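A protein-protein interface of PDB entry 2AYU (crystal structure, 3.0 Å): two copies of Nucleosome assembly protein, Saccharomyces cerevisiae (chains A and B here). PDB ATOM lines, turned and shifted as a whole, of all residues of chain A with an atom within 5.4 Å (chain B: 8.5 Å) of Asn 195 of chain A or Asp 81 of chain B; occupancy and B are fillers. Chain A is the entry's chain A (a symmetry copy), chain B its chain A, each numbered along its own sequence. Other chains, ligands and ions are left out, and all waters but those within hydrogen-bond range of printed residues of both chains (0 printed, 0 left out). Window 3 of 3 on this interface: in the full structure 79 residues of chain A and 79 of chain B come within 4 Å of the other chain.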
ATOM      1  N   LEU A 190     -14.097 -17.350 -19.268  1.00  0.00           N
ATOM      2  CA  LEU A 190     -13.361 -18.314 -20.081  1.00  0.00           C
ATOM      3  C   LEU A 190     -11.879 -18.101 -19.780  1.00  0.00           C
ATOM      4  O   LEU A 190     -11.175 -19.039 -19.414  1.00  0.00           O
ATOM      5  CB  LEU A 190     -13.641 -18.098 -21.574  1.00  0.00           C
ATOM      6  CG  LEU A 190     -12.897 -18.968 -22.605  1.00  0.00           C
ATOM      7  CD1 LEU A 190     -11.422 -18.583 -22.643  1.00  0.00           C
ATOM      8  CD2 LEU A 190     -13.050 -20.437 -22.267  1.00  0.00           C
ATOM      9  N   THR A 191     -11.430 -16.856 -19.919  1.00  0.00           N
ATOM     10  CA  THR A 191     -10.045 -16.460 -19.662  1.00  0.00           C
ATOM     11  C   THR A 191      -9.567 -16.798 -18.251  1.00  0.00           C
ATOM     12  O   THR A 191      -8.456 -17.294 -18.064  1.00  0.00           O
ATOM     13  CB  THR A 191      -9.869 -14.944 -19.868  1.00  0.00           C
ATOM     14  OG1 THR A 191      -9.949 -14.641 -21.267  1.00  0.00           O
ATOM     15  CG2 THR A 191      -8.536 -14.475 -19.295  1.00  0.00           C
ATOM     16  N   ALA A 192     -10.400 -16.502 -17.261  1.00  0.00           N
ATOM     17  CA  ALA A 192     -10.062 -16.780 -15.873  1.00  0.00           C
ATOM     18  C   ALA A 192      -9.858 -18.279 -15.653  1.00  0.00           C
ATOM     19  O   ALA A 192      -8.894 -18.696 -15.011  1.00  0.00           O
ATOM     20  CB  ALA A 192     -11.164 -16.267 -14.959  1.00  0.00           C
ATOM     21  N   LEU A 193     -10.776 -19.081 -16.182  1.00  0.00           N
ATOM     22  CA  LEU A 193     -10.710 -20.534 -16.043  1.00  0.00           C
ATOM     23  C   LEU A 193      -9.489 -21.149 -16.735  1.00  0.00           C
ATOM     24  O   LEU A 193      -8.964 -22.171 -16.291  1.00  0.00           O
ATOM     25  CB  LEU A 193     -11.993 -21.168 -16.592  1.00  0.00           C
ATOM     26  CG  LEU A 193     -13.270 -21.020 -15.758  1.00  0.00           C
ATOM     27  CD1 LEU A 193     -14.448 -21.492 -16.605  1.00  0.00           C
ATOM     28  CD2 LEU A 193     -13.155 -21.819 -14.442  1.00  0.00           C
ATOM     29  N   GLU A 194      -9.050 -20.531 -17.825  1.00  0.00           N
ATOM     30  CA  GLU A 194      -7.883 -21.006 -18.551  1.00  0.00           C
ATOM     31  C   GLU A 194      -6.715 -20.966 -17.580  1.00  0.00           C
ATOM     32  O   GLU A 194      -6.033 -21.964 -17.376  1.00  0.00           O
ATOM     33  CB  GLU A 194      -7.571 -20.083 -19.721  1.00  0.00           C
ATOM     34  CG  GLU A 194      -8.747 -19.809 -20.641  1.00  0.00           C
ATOM     35  CD  GLU A 194      -8.972 -20.913 -21.649  1.00  0.00           C
ATOM     36  OE1 GLU A 194      -8.731 -22.088 -21.286  1.00  0.00           O
ATOM     37  OE2 GLU A 194      -9.395 -20.602 -22.789  1.00  0.00           O
ATOM     38  N   ASN A 195      -6.494 -19.803 -16.973  1.00  0.00           N
ATOM     39  CA  ASN A 195      -5.394 -19.625 -16.025  1.00  0.00           C
ATOM     40  C   ASN A 195      -5.559 -20.397 -14.720  1.00  0.00           C
ATOM     41  O   ASN A 195      -4.715 -20.290 -13.825  1.00  0.00           O
ATOM     42  CB  ASN A 195      -5.217 -18.151 -15.690  1.00  0.00           C
ATOM     43  CG  ASN A 195      -4.880 -17.319 -16.891  1.00  0.00           C
ATOM     44  OD1 ASN A 195      -5.107 -16.110 -16.891  1.00  0.00           O
ATOM     45  ND2 ASN A 195      -4.325 -17.949 -17.923  1.00  0.00           N
ATOM     46  N   LEU A 196      -6.636 -21.162 -14.591  1.00  0.00           N
ATOM     47  CA  LEU A 196      -6.842 -21.939 -13.357  1.00  0.00           C
ATOM     48  C   LEU A 196      -6.351 -23.335 -13.477  1.00  0.00           C
ATOM     49  O   LEU A 196      -6.654 -24.075 -14.410  1.00  0.00           O
ATOM     50  CB  LEU A 196      -8.285 -21.947 -12.919  1.00  0.00           C
ATOM     51  CG  LEU A 196      -8.507 -22.604 -11.571  1.00  0.00           C
ATOM     52  CD1 LEU A 196      -7.757 -21.862 -10.477  1.00  0.00           C
ATOM     53  CD2 LEU A 196      -9.992 -22.685 -11.244  1.00  0.00           C
ATOM     54  N   PRO A 197      -5.606 -23.658 -12.491  1.00  0.00           N
ATOM     55  CA  PRO A 197      -5.130 -24.989 -12.571  1.00  0.00           C
ATOM     56  C   PRO A 197      -6.303 -25.938 -12.685  1.00  0.00           C
ATOM     57  O   PRO A 197      -7.463 -25.605 -12.429  1.00  0.00           O
ATOM     58  CB  PRO A 197      -4.315 -25.135 -11.298  1.00  0.00           C
ATOM     59  CG  PRO A 197      -3.530 -23.875 -11.338  1.00  0.00           C
ATOM     60  CD  PRO A 197      -4.306 -22.973 -12.264  1.00  0.00           C
ATOM     61  N   CYS A 200      -8.336 -25.844 -16.576  1.00  0.00           N
ATOM     62  CA  CYS A 200      -7.895 -25.469 -17.926  1.00  0.00           C
ATOM     63  C   CYS A 200      -7.651 -26.626 -18.893  1.00  0.00           C
ATOM     64  O   CYS A 200      -7.656 -26.446 -20.115  1.00  0.00           O
ATOM     65  CB  CYS A 200      -6.619 -24.645 -17.827  1.00  0.00           C
ATOM     66  SG  CYS A 200      -5.461 -25.300 -16.597  1.00  0.00           S
ATOM     67  N   TRP A 359      -7.572 -14.246 -11.476  1.00  0.00           N
ATOM     68  CA  TRP A 359      -7.408 -15.414 -12.321  1.00  0.00           C
ATOM     69  C   TRP A 359      -7.498 -15.021 -13.780  1.00  0.00           C
ATOM     70  O   TRP A 359      -7.035 -15.736 -14.661  1.00  0.00           O
ATOM     71  CB  TRP A 359      -8.444 -16.476 -11.975  1.00  0.00           C
ATOM     72  CG  TRP A 359      -8.014 -17.150 -10.768  1.00  0.00           C
ATOM     73  CD1 TRP A 359      -8.431 -16.900  -9.499  1.00  0.00           C
ATOM     74  CD2 TRP A 359      -6.900 -18.037 -10.661  1.00  0.00           C
ATOM     75  NE1 TRP A 359      -7.631 -17.564  -8.600  1.00  0.00           N
ATOM     76  CE2 TRP A 359      -6.681 -18.271  -9.291  1.00  0.00           C
ATOM     77  CE3 TRP A 359      -6.056 -18.652 -11.595  1.00  0.00           C
ATOM     78  CZ2 TRP A 359      -5.648 -19.095  -8.827  1.00  0.00           C
ATOM     79  CZ3 TRP A 359      -5.026 -19.472 -11.135  1.00  0.00           C
ATOM     80  CH2 TRP A 359      -4.833 -19.683  -9.763  1.00  0.00           C
ATOM     81  N   PHE A 360      -8.092 -13.864 -14.031  1.00  0.00           N
ATOM     82  CA  PHE A 360      -8.213 -13.372 -15.384  1.00  0.00           C
ATOM     83  C   PHE A 360      -6.859 -12.773 -15.755  1.00  0.00           C
ATOM     84  O   PHE A 360      -6.286 -13.110 -16.791  1.00  0.00           O
ATOM     85  CB  PHE A 360      -9.311 -12.319 -15.449  1.00  0.00           C
ATOM     86  CG  PHE A 360      -9.405 -11.640 -16.768  1.00  0.00           C
ATOM     87  CD1 PHE A 360      -8.576 -10.563 -17.064  1.00  0.00           C
ATOM     88  CD2 PHE A 360     -10.282 -12.114 -17.743  1.00  0.00           C
ATOM     89  CE1 PHE A 360      -8.609  -9.970 -18.312  1.00  0.00           C
ATOM     90  CE2 PHE A 360     -10.327 -11.530 -19.000  1.00  0.00           C
ATOM     91  CZ  PHE A 360      -9.488 -10.454 -19.290  1.00  0.00           C
ATOM     92  N   THR A 361      -6.346 -11.898 -14.891  1.00  0.00           N
ATOM     93  CA  THR A 361      -5.052 -11.253 -15.108  1.00  0.00           C
ATOM     94  C   THR A 361      -3.882 -12.225 -14.965  1.00  0.00           C
ATOM     95  O   THR A 361      -2.772 -11.934 -15.410  1.00  0.00           O
ATOM     96  CB  THR A 361      -4.812 -10.064 -14.115  1.00  0.00           C
ATOM     97  OG1 THR A 361      -5.033 -10.485 -12.762  1.00  0.00           O
ATOM     98  CG2 THR A 361      -5.728  -8.909 -14.439  1.00  0.00           C
ATOM     99  N   GLY A 362      -4.129 -13.382 -14.359  1.00  0.00           N
ATOM    100  CA  GLY A 362      -3.059 -14.347 -14.153  1.00  0.00           C
ATOM    101  C   GLY A 362      -2.320 -13.979 -12.875  1.00  0.00           C
ATOM    102  O   GLY A 362      -1.506 -14.748 -12.347  1.00  0.00           O
ATOM    103  N   LEU A 365      -2.229 -16.537  -9.951  1.00  0.00           N
ATOM    104  CA  LEU A 365      -1.161 -17.557  -9.983  1.00  0.00           C
ATOM    105  C   LEU A 365       0.042 -17.157  -9.132  1.00  0.00           C
ATOM    106  O   LEU A 365       0.501 -17.909  -8.269  1.00  0.00           O
ATOM    107  CB  LEU A 365      -0.687 -17.806 -11.431  1.00  0.00           C
ATOM    108  CG  LEU A 365      -1.597 -18.551 -12.433  1.00  0.00           C
ATOM    109  CD1 LEU A 365      -1.105 -18.333 -13.860  1.00  0.00           C
ATOM    110  CD2 LEU A 365      -1.645 -20.043 -12.112  1.00  0.00           C
ATOM    111  N   ARG B  73       7.186 -21.331 -14.597  1.00  0.00           N
ATOM    112  CA  ARG B  73       5.762 -21.435 -14.897  1.00  0.00           C
ATOM    113  C   ARG B  73       5.048 -20.147 -14.460  1.00  0.00           C
ATOM    114  O   ARG B  73       3.817 -20.071 -14.490  1.00  0.00           O
ATOM    115  CB  ARG B  73       5.147 -22.630 -14.166  1.00  0.00           C
ATOM    116  CG  ARG B  73       5.733 -23.995 -14.528  1.00  0.00           C
ATOM    117  CD  ARG B  73       4.935 -25.097 -13.826  1.00  0.00           C
ATOM    118  NE  ARG B  73       5.421 -26.447 -14.109  1.00  0.00           N
ATOM    119  CZ  ARG B  73       4.799 -27.561 -13.722  1.00  0.00           C
ATOM    120  NH1 ARG B  73       3.662 -27.495 -13.033  1.00  0.00           N
ATOM    121  NH2 ARG B  73       5.312 -28.748 -14.025  1.00  0.00           N
ATOM    122  N   LEU B  74       5.833 -19.152 -14.041  1.00  0.00           N
ATOM    123  CA  LEU B  74       5.320 -17.852 -13.605  1.00  0.00           C
ATOM    124  C   LEU B  74       6.100 -16.717 -14.264  1.00  0.00           C
ATOM    125  O   LEU B  74       5.735 -15.543 -14.160  1.00  0.00           O
ATOM    126  CB  LEU B  74       5.380 -17.714 -12.073  1.00  0.00           C
ATOM    127  CG  LEU B  74       6.319 -18.556 -11.207  1.00  0.00           C
ATOM    128  CD1 LEU B  74       6.364 -17.973  -9.799  1.00  0.00           C
ATOM    129  CD2 LEU B  74       5.840 -20.003 -11.173  1.00  0.00           C
ATOM    130  N   GLY B  75       7.187 -17.077 -14.935  1.00  0.00           N
ATOM    131  CA  GLY B  75       7.976 -16.079 -15.627  1.00  0.00           C
ATOM    132  C   GLY B  75       7.477 -16.041 -17.057  1.00  0.00           C
ATOM    133  O   GLY B  75       7.470 -14.995 -17.710  1.00  0.00           O
ATOM    134  N   SER B  76       7.044 -17.205 -17.535  1.00  0.00           N
ATOM    135  CA  SER B  76       6.517 -17.359 -18.885  1.00  0.00           C
ATOM    136  C   SER B  76       4.997 -17.224 -18.847  1.00  0.00           C
ATOM    137  O   SER B  76       4.404 -16.525 -19.673  1.00  0.00           O
ATOM    138  CB  SER B  76       6.893 -18.735 -19.448  1.00  0.00           C
ATOM    139  OG  SER B  76       6.287 -19.779 -18.701  1.00  0.00           O
ATOM    140  N   LEU B  77       4.375 -17.897 -17.882  1.00  0.00           N
ATOM    141  CA  LEU B  77       2.925 -17.848 -17.743  1.00  0.00           C
ATOM    142  C   LEU B  77       2.504 -16.430 -17.368  1.00  0.00           C
ATOM    143  O   LEU B  77       1.996 -15.698 -18.217  1.00  0.00           O
ATOM    144  CB  LEU B  77       2.442 -18.842 -16.674  1.00  0.00           C
ATOM    145  CG  LEU B  77       1.188 -19.682 -16.984  1.00  0.00           C
ATOM    146  CD1 LEU B  77       0.884 -20.594 -15.802  1.00  0.00           C
ATOM    147  CD2 LEU B  77      -0.008 -18.785 -17.283  1.00  0.00           C
ATOM    148  N   VAL B  78       2.726 -16.036 -16.113  1.00  0.00           N
ATOM    149  CA  VAL B  78       2.347 -14.695 -15.667  1.00  0.00           C
ATOM    150  C   VAL B  78       2.805 -13.644 -16.674  1.00  0.00           C
ATOM    151  O   VAL B  78       2.235 -12.551 -16.744  1.00  0.00           O
ATOM    152  CB  VAL B  78       2.943 -14.350 -14.277  1.00  0.00           C
ATOM    153  CG1 VAL B  78       2.513 -12.941 -13.868  1.00  0.00           C
ATOM    154  CG2 VAL B  78       2.468 -15.355 -13.235  1.00  0.00           C
ATOM    155  N   GLY B  79       3.830 -13.993 -17.452  1.00  0.00           N
ATOM    156  CA  GLY B  79       4.352 -13.092 -18.465  1.00  0.00           C
ATOM    157  C   GLY B  79       3.342 -12.801 -19.565  1.00  0.00           C
ATOM    158  O   GLY B  79       2.938 -11.651 -19.766  1.00  0.00           O
ATOM    159  N   GLN B  80       2.938 -13.836 -20.292  1.00  0.00           N
ATOM    160  CA  GLN B  80       1.961 -13.660 -21.355  1.00  0.00           C
ATOM    161  C   GLN B  80       0.670 -13.102 -20.753  1.00  0.00           C
ATOM    162  O   GLN B  80       0.043 -12.216 -21.339  1.00  0.00           O
ATOM    163  CB  GLN B  80       1.663 -14.994 -22.034  1.00  0.00           C
ATOM    164  CG  GLN B  80       2.884 -15.773 -22.479  1.00  0.00           C
ATOM    165  CD  GLN B  80       2.499 -17.098 -23.102  1.00  0.00           C
ATOM    166  OE1 GLN B  80       1.888 -17.138 -24.174  1.00  0.00           O
ATOM    167  NE2 GLN B  80       2.841 -18.193 -22.426  1.00  0.00           N
ATOM    168  N   ASP B  81       0.287 -13.625 -19.585  1.00  0.00           N
ATOM    169  CA  ASP B  81      -0.924 -13.185 -18.890  1.00  0.00           C
ATOM    170  C   ASP B  81      -0.864 -11.689 -18.660  1.00  0.00           C
ATOM    171  O   ASP B  81      -1.704 -10.948 -19.165  1.00  0.00           O
ATOM    172  CB  ASP B  81      -1.081 -13.901 -17.546  1.00  0.00           C
ATOM    173  CG  ASP B  81      -1.388 -15.386 -17.702  1.00  0.00           C
ATOM    174  OD1 ASP B  81      -1.795 -15.801 -18.810  1.00  0.00           O
ATOM    175  OD2 ASP B  81      -1.236 -16.143 -16.716  1.00  0.00           O
ATOM    176  N   SER B  82       0.137 -11.249 -17.903  1.00  0.00           N
ATOM    177  CA  SER B  82       0.324  -9.824 -17.616  1.00  0.00           C
ATOM    178  C   SER B  82       0.441  -9.026 -18.936  1.00  0.00           C
ATOM    179  O   SER B  82       0.306  -7.797 -18.960  1.00  0.00           O
ATOM    180  CB  SER B  82       1.579  -9.640 -16.746  1.00  0.00           C
ATOM    181  OG  SER B  82       1.635  -8.356 -16.146  1.00  0.00           O
ATOM    182  N   GLY B  83       0.684  -9.745 -20.029  1.00  0.00           N
ATOM    183  CA  GLY B  83       0.803  -9.112 -21.328  1.00  0.00           C
ATOM    184  C   GLY B  83      -0.559  -8.983 -21.978  1.00  0.00           C
ATOM    185  O   GLY B  83      -0.963  -7.890 -22.373  1.00  0.00           O
ATOM    186  N   TYR B  84      -1.263 -10.106 -22.098  1.00  0.00           N
ATOM    187  CA  TYR B  84      -2.593 -10.112 -22.687  1.00  0.00           C
ATOM    188  C   TYR B  84      -3.337  -8.932 -22.093  1.00  0.00           C
ATOM    189  O   TYR B  84      -3.776  -8.034 -22.813  1.00  0.00           O
ATOM    190  CB  TYR B  84      -3.332 -11.403 -22.328  1.00  0.00           C
ATOM    191  CG  TYR B  84      -4.758 -11.490 -22.845  1.00  0.00           C
ATOM    192  CD1 TYR B  84      -5.022 -11.601 -24.211  1.00  0.00           C
ATOM    193  CD2 TYR B  84      -5.846 -11.504 -21.963  1.00  0.00           C
ATOM    194  CE1 TYR B  84      -6.342 -11.733 -24.695  1.00  0.00           C
ATOM    195  CE2 TYR B  84      -7.172 -11.634 -22.432  1.00  0.00           C
ATOM    196  CZ  TYR B  84      -7.413 -11.750 -23.801  1.00  0.00           C
ATOM    197  OH  TYR B  84      -8.706 -11.902 -24.273  1.00  0.00           O
ATOM    198  N   VAL B  85      -3.452  -8.945 -20.765  1.00  0.00           N
ATOM    199  CA  VAL B  85      -4.140  -7.894 -20.022  1.00  0.00           C
ATOM    200  C   VAL B  85      -3.564  -6.539 -20.364  1.00  0.00           C
ATOM    201  O   VAL B  85      -4.301  -5.560 -20.497  1.00  0.00           O
ATOM    202  CB  VAL B  85      -4.040  -8.115 -18.490  1.00  0.00           C
ATOM    203  CG1 VAL B  85      -2.647  -8.535 -18.124  1.00  0.00           C
ATOM    204  CG2 VAL B  85      -4.398  -6.830 -17.742  1.00  0.00           C
ATOM    205  N   GLY B  86      -2.244  -6.486 -20.503  1.00  0.00           N
ATOM    206  CA  GLY B  86      -1.602  -5.233 -20.845  1.00  0.00           C
ATOM    207  C   GLY B  86      -2.129  -4.672 -22.160  1.00  0.00           C
ATOM    208  O   GLY B  86      -2.241  -3.452 -22.323  1.00  0.00           O
ATOM    209  N   GLY B  87      -2.466  -5.562 -23.095  1.00  0.00           N
ATOM    210  CA  GLY B  87      -2.963  -5.130 -24.391  1.00  0.00           C
ATOM    211  C   GLY B  87      -4.447  -4.818 -24.514  1.00  0.00           C
ATOM    212  O   GLY B  87      -4.878  -4.264 -25.522  1.00  0.00           O
ATOM    213  N   LEU B  88      -5.238  -5.164 -23.506  1.00  0.00           N
ATOM    214  CA  LEU B  88      -6.671  -4.900 -23.562  1.00  0.00           C
ATOM    215  C   LEU B  88      -6.983  -3.403 -23.760  1.00  0.00           C
ATOM    216  O   LEU B  88      -6.159  -2.534 -23.450  1.00  0.00           O
ATOM    217  CB  LEU B  88      -7.343  -5.421 -22.284  1.00  0.00           C
ATOM    218  CG  LEU B  88      -7.120  -6.893 -21.911  1.00  0.00           C
ATOM    219  CD1 LEU B  88      -7.889  -7.209 -20.636  1.00  0.00           C
ATOM    220  CD2 LEU B  88      -7.578  -7.805 -23.037  1.00  0.00           C
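OD1 of Asp 81 of chain B is in hydrogen-bond range of ND2 of Asn 195 of chain A, at 3.4 Å.
No position is printed for both chains.
The side-chain amide oxygen (OD1) of Asn 195 of chain A lies close to the backbone carbonyl oxygen (O) of Trp 359 of chain A (3.0 Å). The side-chain amide oxygen (OD1) of Asn 195 of chain A lies close to the backbone carbonyl oxygen (O) of Phe 360 of chain A (3.2 Å).
Of chain B, only Asp 81 comes within 4 Å of Asn 195 of chain A. Of the printed residues of chain B, Phe 360 of chain A touches Leu 88 (3.7 Å). Of the printed residues of chain A, Leu 77 of chain B touches Leu 365. Of the printed residues of chain B, Gly 362 of chain A touches Asp 81 (3.6 Å). Of the printed residues of chain B, Leu 365 of chain A touches Leu 77 (3.6 Å) and Asp 81 (3.6 Å). Of the printed residues of chain A, Leu 88 of chain B touches Phe 360 (3.7 Å). The nearest residue of chain A that does not touch Asp 81 of chain B is Phe 360 of chain A (5.3 Å).
Among the printed residues, merely in contact across the chains: Phe 360 of chain A with Leu 88 of chain B, Thr 361 of chain A with Asp 81 of chain B, Thr 361 of chain A with Ser 82 of chain B, Gly 362 of chain A with Asp 81 of chain B, Leu 365 of chain A with Leu 77 of chain B and Leu 365 of chain A with Asp 81 of chain B.
Of the 14 printed residues of chain A, 5 touch a printed residue of chain B. Printed residues of chain A that touch a printed residue of chain B: Asn 195, Phe 360, Thr 361, Gly 362 and Leu 365. Hydrophobic or aromatic side chains of chain A that line the printed part of chain B: Phe 360 and Leu 365. Hydrophobic or aromatic side chains of chain B that line the printed part of chain A: Leu 77 and Leu 88. Along chain B the printed residues that touch a printed residue of chain A span positions 77 to 88. Among the printed residues, no Asp or Glu carboxylate lies within 4 Å of a Lys or Arg side-chain nitrogen of the other chain.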
